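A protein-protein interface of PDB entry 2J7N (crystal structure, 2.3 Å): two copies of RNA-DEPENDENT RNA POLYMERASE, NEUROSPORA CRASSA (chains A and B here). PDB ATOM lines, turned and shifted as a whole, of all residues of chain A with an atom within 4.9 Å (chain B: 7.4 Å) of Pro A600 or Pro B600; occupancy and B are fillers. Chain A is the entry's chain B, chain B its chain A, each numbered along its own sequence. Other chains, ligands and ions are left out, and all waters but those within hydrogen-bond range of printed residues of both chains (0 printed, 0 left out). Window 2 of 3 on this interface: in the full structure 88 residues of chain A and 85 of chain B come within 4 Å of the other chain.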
ATOM      1  N   SER A 574       6.849  19.798  -3.359  1.00  0.00           N
ATOM      2  CA  SER A 574       6.643  18.848  -4.452  1.00  0.00           C
ATOM      3  C   SER A 574       6.942  19.469  -5.804  1.00  0.00           C
ATOM      4  O   SER A 574       6.557  20.599  -6.056  1.00  0.00           O
ATOM      5  CB  SER A 574       5.199  18.365  -4.441  1.00  0.00           C
ATOM      6  OG  SER A 574       5.093  17.100  -5.040  1.00  0.00           O
ATOM      7  N   PHE A 598       7.190  14.620  -3.426  1.00  0.00           N
ATOM      8  CA  PHE A 598       6.342  14.138  -2.349  1.00  0.00           C
ATOM      9  C   PHE A 598       5.846  12.711  -2.638  1.00  0.00           C
ATOM     10  O   PHE A 598       5.129  12.461  -3.615  1.00  0.00           O
ATOM     11  CB  PHE A 598       5.159  15.094  -2.152  1.00  0.00           C
ATOM     12  CG  PHE A 598       4.375  14.843  -0.893  1.00  0.00           C
ATOM     13  CD1 PHE A 598       4.752  15.433   0.310  1.00  0.00           C
ATOM     14  CD2 PHE A 598       3.253  14.029  -0.911  1.00  0.00           C
ATOM     15  CE1 PHE A 598       4.035  15.196   1.464  1.00  0.00           C
ATOM     16  CE2 PHE A 598       2.532  13.789   0.261  1.00  0.00           C
ATOM     17  CZ  PHE A 598       2.912  14.370   1.439  1.00  0.00           C
ATOM     18  N   LYS A 599       6.242  11.778  -1.777  1.00  0.00           N
ATOM     19  CA  LYS A 599       5.857  10.379  -1.881  1.00  0.00           C
ATOM     20  C   LYS A 599       4.719  10.142  -0.901  1.00  0.00           C
ATOM     21  O   LYS A 599       4.874  10.353   0.295  1.00  0.00           O
ATOM     22  CB  LYS A 599       7.055   9.483  -1.553  1.00  0.00           C
ATOM     23  CG  LYS A 599       8.285   9.785  -2.376  1.00  0.00           C
ATOM     24  CD  LYS A 599       8.061   9.344  -3.819  1.00  0.00           C
ATOM     25  CE  LYS A 599       9.379   9.306  -4.604  1.00  0.00           C
ATOM     26  NZ  LYS A 599       9.208   8.909  -6.051  1.00  0.00           N
ATOM     27  N   PRO A 600       3.552   9.741  -1.415  1.00  0.00           N
ATOM     28  CA  PRO A 600       2.396   9.476  -0.562  1.00  0.00           C
ATOM     29  C   PRO A 600       2.621   8.371   0.472  1.00  0.00           C
ATOM     30  O   PRO A 600       2.032   8.433   1.549  1.00  0.00           O
ATOM     31  CB  PRO A 600       1.288   9.119  -1.563  1.00  0.00           C
ATOM     32  CG  PRO A 600       1.749   9.724  -2.871  1.00  0.00           C
ATOM     33  CD  PRO A 600       3.244   9.550  -2.841  1.00  0.00           C
ATOM     34  N   GLU A 601       3.492   7.401   0.178  1.00  0.00           N
ATOM     35  CA  GLU A 601       3.913   6.419   1.196  1.00  0.00           C
ATOM     36  C   GLU A 601       4.522   7.076   2.441  1.00  0.00           C
ATOM     37  O   GLU A 601       4.413   6.527   3.532  1.00  0.00           O
ATOM     38  CB  GLU A 601       4.911   5.382   0.648  1.00  0.00           C
ATOM     39  CG  GLU A 601       4.516   4.732  -0.686  1.00  0.00           C
ATOM     40  CD  GLU A 601       4.866   5.615  -1.879  1.00  0.00           C
ATOM     41  OE1 GLU A 601       4.751   6.852  -1.764  1.00  0.00           O
ATOM     42  OE2 GLU A 601       5.260   5.079  -2.930  1.00  0.00           O
ATOM     43  N   LEU A 602       5.146   8.249   2.282  1.00  0.00           N
ATOM     44  CA  LEU A 602       5.821   8.918   3.400  1.00  0.00           C
ATOM     45  C   LEU A 602       5.014  10.069   3.971  1.00  0.00           C
ATOM     46  O   LEU A 602       5.530  10.847   4.793  1.00  0.00           O
ATOM     47  CB  LEU A 602       7.196   9.433   2.977  1.00  0.00           C
ATOM     48  CG  LEU A 602       8.070   8.398   2.261  1.00  0.00           C
ATOM     49  CD1 LEU A 602       9.411   8.998   1.872  1.00  0.00           C
ATOM     50  CD2 LEU A 602       8.244   7.158   3.139  1.00  0.00           C
ATOM     51  N   HIS A 603       3.760  10.178   3.550  1.00  0.00           N
ATOM     52  CA  HIS A 603       2.940  11.344   3.868  1.00  0.00           C
ATOM     53  C   HIS A 603       2.834  11.631   5.351  1.00  0.00           C
ATOM     54  O   HIS A 603       2.645  12.770   5.728  1.00  0.00           O
ATOM     55  CB  HIS A 603       1.534  11.224   3.285  1.00  0.00           C
ATOM     56  CG  HIS A 603       0.603  10.387   4.107  1.00  0.00           C
ATOM     57  ND1 HIS A 603       0.461   9.025   3.917  1.00  0.00           N
ATOM     58  CD2 HIS A 603      -0.253  10.719   5.103  1.00  0.00           C
ATOM     59  CE1 HIS A 603      -0.424   8.550   4.777  1.00  0.00           C
ATOM     60  NE2 HIS A 603      -0.880   9.558   5.500  1.00  0.00           N
ATOM     61  N   VAL B 370      -3.843  22.981 -12.118  1.00  0.00           N
ATOM     62  CA  VAL B 370      -2.555  22.524 -11.599  1.00  0.00           C
ATOM     63  C   VAL B 370      -1.460  22.447 -12.686  1.00  0.00           C
ATOM     64  O   VAL B 370      -0.279  22.489 -12.383  1.00  0.00           O
ATOM     65  CB  VAL B 370      -2.662  21.185 -10.830  1.00  0.00           C
ATOM     66  CG1 VAL B 370      -3.747  21.276  -9.795  1.00  0.00           C
ATOM     67  CG2 VAL B 370      -2.913  20.020 -11.755  1.00  0.00           C
ATOM     68  N   VAL B 549      -6.739  11.807 -12.566  1.00  0.00           N
ATOM     69  CA  VAL B 549      -5.853  11.090 -11.653  1.00  0.00           C
ATOM     70  C   VAL B 549      -6.609  10.277 -10.609  1.00  0.00           C
ATOM     71  O   VAL B 549      -6.081   9.304 -10.071  1.00  0.00           O
ATOM     72  CB  VAL B 549      -4.794  12.038 -10.984  1.00  0.00           C
ATOM     73  CG1 VAL B 549      -3.783  12.531 -12.018  1.00  0.00           C
ATOM     74  CG2 VAL B 549      -5.454  13.238 -10.291  1.00  0.00           C
ATOM     75  N   HIS B 556      -9.674  13.349  -3.316  1.00  0.00           N
ATOM     76  CA  HIS B 556      -8.433  13.952  -2.891  1.00  0.00           C
ATOM     77  C   HIS B 556      -8.752  15.119  -1.952  1.00  0.00           C
ATOM     78  O   HIS B 556      -9.514  15.992  -2.310  1.00  0.00           O
ATOM     79  CB  HIS B 556      -7.630  14.430  -4.100  1.00  0.00           C
ATOM     80  CG  HIS B 556      -6.389  15.187  -3.735  1.00  0.00           C
ATOM     81  ND1 HIS B 556      -5.125  14.643  -3.841  1.00  0.00           N
ATOM     82  CD2 HIS B 556      -6.217  16.449  -3.262  1.00  0.00           C
ATOM     83  CE1 HIS B 556      -4.231  15.539  -3.456  1.00  0.00           C
ATOM     84  NE2 HIS B 556      -4.867  16.640  -3.093  1.00  0.00           N
ATOM     85  N   LEU B 572      -3.595  16.638   5.484  1.00  0.00           N
ATOM     86  CA  LEU B 572      -4.212  16.036   4.326  1.00  0.00           C
ATOM     87  C   LEU B 572      -4.811  14.694   4.694  1.00  0.00           C
ATOM     88  O   LEU B 572      -4.653  14.222   5.816  1.00  0.00           O
ATOM     89  CB  LEU B 572      -3.203  15.915   3.169  1.00  0.00           C
ATOM     90  CG  LEU B 572      -2.056  14.903   2.917  1.00  0.00           C
ATOM     91  CD1 LEU B 572      -0.633  15.504   3.021  1.00  0.00           C
ATOM     92  CD2 LEU B 572      -2.163  13.501   3.534  1.00  0.00           C
ATOM     93  N   SER B 574      -5.196  10.650   3.551  1.00  0.00           N
ATOM     94  CA  SER B 574      -4.634   9.645   2.685  1.00  0.00           C
ATOM     95  C   SER B 574      -4.731   8.260   3.279  1.00  0.00           C
ATOM     96  O   SER B 574      -4.542   8.059   4.496  1.00  0.00           O
ATOM     97  CB  SER B 574      -3.177   9.952   2.363  1.00  0.00           C
ATOM     98  OG  SER B 574      -2.703   9.105   1.329  1.00  0.00           O
ATOM     99  N   ASP B 575      -4.996   7.303   2.388  1.00  0.00           N
ATOM    100  CA  ASP B 575      -5.207   5.891   2.730  1.00  0.00           C
ATOM    101  C   ASP B 575      -6.157   5.584   3.864  1.00  0.00           C
ATOM    102  O   ASP B 575      -5.848   4.836   4.770  1.00  0.00           O
ATOM    103  CB  ASP B 575      -3.898   5.116   2.860  1.00  0.00           C
ATOM    104  CG  ASP B 575      -3.542   4.388   1.558  1.00  0.00           C
ATOM    105  OD1 ASP B 575      -3.517   5.069   0.493  1.00  0.00           O
ATOM    106  OD2 ASP B 575      -3.348   3.142   1.589  1.00  0.00           O
ATOM    107  N   VAL B 597      -7.536   9.363  -1.115  1.00  0.00           N
ATOM    108  CA  VAL B 597      -6.256   9.050  -1.743  1.00  0.00           C
ATOM    109  C   VAL B 597      -5.540  10.315  -2.198  1.00  0.00           C
ATOM    110  O   VAL B 597      -5.988  10.980  -3.131  1.00  0.00           O
ATOM    111  CB  VAL B 597      -6.467   8.197  -2.989  1.00  0.00           C
ATOM    112  CG1 VAL B 597      -5.130   7.833  -3.621  1.00  0.00           C
ATOM    113  CG2 VAL B 597      -7.232   6.950  -2.638  1.00  0.00           C
ATOM    114  N   PHE B 598      -4.413  10.635  -1.576  1.00  0.00           N
ATOM    115  CA  PHE B 598      -3.747  11.886  -1.863  1.00  0.00           C
ATOM    116  C   PHE B 598      -2.950  11.739  -3.138  1.00  0.00           C
ATOM    117  O   PHE B 598      -2.093  10.874  -3.226  1.00  0.00           O
ATOM    118  CB  PHE B 598      -2.809  12.288  -0.706  1.00  0.00           C
ATOM    119  CG  PHE B 598      -2.300  13.686  -0.818  1.00  0.00           C
ATOM    120  CD1 PHE B 598      -3.079  14.758  -0.387  1.00  0.00           C
ATOM    121  CD2 PHE B 598      -1.066  13.945  -1.400  1.00  0.00           C
ATOM    122  CE1 PHE B 598      -2.622  16.056  -0.523  1.00  0.00           C
ATOM    123  CE2 PHE B 598      -0.609  15.234  -1.536  1.00  0.00           C
ATOM    124  CZ  PHE B 598      -1.389  16.291  -1.102  1.00  0.00           C
ATOM    125  N   LYS B 599      -3.240  12.582  -4.125  1.00  0.00           N
ATOM    126  CA  LYS B 599      -2.509  12.588  -5.385  1.00  0.00           C
ATOM    127  C   LYS B 599      -1.537  13.765  -5.389  1.00  0.00           C
ATOM    128  O   LYS B 599      -1.942  14.918  -5.267  1.00  0.00           O
ATOM    129  CB  LYS B 599      -3.458  12.684  -6.589  1.00  0.00           C
ATOM    130  CG  LYS B 599      -4.576  11.641  -6.581  1.00  0.00           C
ATOM    131  CD  LYS B 599      -4.046  10.248  -6.928  1.00  0.00           C
ATOM    132  CE  LYS B 599      -5.163   9.217  -6.892  1.00  0.00           C
ATOM    133  NZ  LYS B 599      -4.866   8.019  -7.760  1.00  0.00           N
ATOM    134  N   PRO B 600      -0.236  13.463  -5.490  1.00  0.00           N
ATOM    135  CA  PRO B 600       0.808  14.481  -5.581  1.00  0.00           C
ATOM    136  C   PRO B 600       0.572  15.505  -6.701  1.00  0.00           C
ATOM    137  O   PRO B 600       0.900  16.684  -6.525  1.00  0.00           O
ATOM    138  CB  PRO B 600       2.076  13.655  -5.840  1.00  0.00           C
ATOM    139  CG  PRO B 600       1.793  12.324  -5.229  1.00  0.00           C
ATOM    140  CD  PRO B 600       0.315  12.093  -5.459  1.00  0.00           C
ATOM    141  N   GLU B 601      -0.007  15.062  -7.819  1.00  0.00           N
ATOM    142  CA  GLU B 601      -0.419  15.957  -8.905  1.00  0.00           C
ATOM    143  C   GLU B 601      -1.378  17.076  -8.451  1.00  0.00           C
ATOM    144  O   GLU B 601      -1.345  18.174  -8.996  1.00  0.00           O
ATOM    145  CB  GLU B 601      -1.076  15.166 -10.053  1.00  0.00           C
ATOM    146  CG  GLU B 601      -0.290  13.932 -10.559  1.00  0.00           C
ATOM    147  CD  GLU B 601      -0.576  12.701  -9.716  1.00  0.00           C
ATOM    148  OE1 GLU B 601      -0.394  12.774  -8.490  1.00  0.00           O
ATOM    149  OE2 GLU B 601      -1.013  11.669 -10.258  1.00  0.00           O
ATOM    150  N   LEU B 602      -2.218  16.790  -7.456  1.00  0.00           N
ATOM    151  CA  LEU B 602      -3.202  17.764  -6.986  1.00  0.00           C
ATOM    152  C   LEU B 602      -2.783  18.409  -5.678  1.00  0.00           C
ATOM    153  O   LEU B 602      -3.573  19.090  -5.048  1.00  0.00           O
ATOM    154  CB  LEU B 602      -4.581  17.099  -6.832  1.00  0.00           C
ATOM    155  CG  LEU B 602      -5.054  16.235  -7.998  1.00  0.00           C
ATOM    156  CD1 LEU B 602      -6.378  15.542  -7.675  1.00  0.00           C
ATOM    157  CD2 LEU B 602      -5.211  17.093  -9.232  1.00  0.00           C
ATOM    158  N   HIS B 603      -1.528  18.207  -5.291  1.00  0.00           N
ATOM    159  CA  HIS B 603      -1.008  18.705  -4.017  1.00  0.00           C
ATOM    160  C   HIS B 603      -1.293  20.185  -3.735  1.00  0.00           C
ATOM    161  O   HIS B 603      -1.444  20.564  -2.582  1.00  0.00           O
ATOM    162  CB  HIS B 603       0.502  18.429  -3.900  1.00  0.00           C
ATOM    163  CG  HIS B 603       1.369  19.416  -4.628  1.00  0.00           C
ATOM    164  ND1 HIS B 603       1.938  19.142  -5.858  1.00  0.00           N
ATOM    165  CD2 HIS B 603       1.786  20.663  -4.288  1.00  0.00           C
ATOM    166  CE1 HIS B 603       2.650  20.184  -6.254  1.00  0.00           C
ATOM    167  NE2 HIS B 603       2.576  21.119  -5.320  1.00  0.00           N
ATOM    168  N   SER B 604      -1.370  21.007  -4.780  1.00  0.00           N
ATOM    169  CA  SER B 604      -1.482  22.466  -4.620  1.00  0.00           C
ATOM    170  C   SER B 604      -2.901  22.929  -4.335  1.00  0.00           C
ATOM    171  O   SER B 604      -3.114  24.084  -3.982  1.00  0.00           O
ATOM    172  CB  SER B 604      -0.987  23.176  -5.883  1.00  0.00           C
ATOM    173  OG  SER B 604      -1.718  22.724  -7.029  1.00  0.00           O
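The backbone carbonyl oxygen (O) of Pro B600 is in hydrogen-bond range of a ring nitrogen (ND1) of His B603 (2.8 Å).
The backbone carbonyl oxygen (O) of Pro A600 lies within hydrogen-bond range of a ring nitrogen (ND1) of His A603 (2.9 Å).
His B603 touches Ser A574 (CE1 to CB, 3.6 Å).
CE2 of Phe A598 touches CE2 of Phe B598, 3.9 Å away.
Pro B600 touches Phe A598 (CG to O, 3.7 Å).
Pro B600 touches Pro A600.
His A603 touches Leu B572 (CD2 to CD2, 3.7 Å).
NE2 of His A603 touches CB of Ser B574 (3.9 Å).
Of chain B, only Pro B600 comes within 4 Å of Pro A600.
Pro B600 touches just these residues of chain A: Phe A598 and Pro A600.
Of the printed residues of chain A, Phe B598 touches Phe A598.
Printed residues of chain B within 4 Å of His A603: Leu B572 and Ser B574.
Asp B575 touches none of the printed residues of chain A.
The nearest residue of chain B that does not touch Pro A600 is Phe B598 (4.03 Å).
The nearest printed residue of chain A that does not touch Ser B574 is Pro A600 (4.8 Å).
Along chain B the printed residues that touch a printed residue of chain A span positions 572 to 603.
Of the 7 printed residues of chain A, 4 touch a printed residue of chain B.
Ser A574 touches His B603, and with the chains exchanged His A603 touches Ser B574.
Phe A598 touches its own counterpart, Phe B598.
Phe A598 touches Pro B600, but with the chains exchanged Pro A600 does not touch Phe B598 (4.03 Å).
Pro B600 touches its own counterpart, Pro A600.
Positions printed for both chains: 574, 598, 599, 600, 601, 602 and 603.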
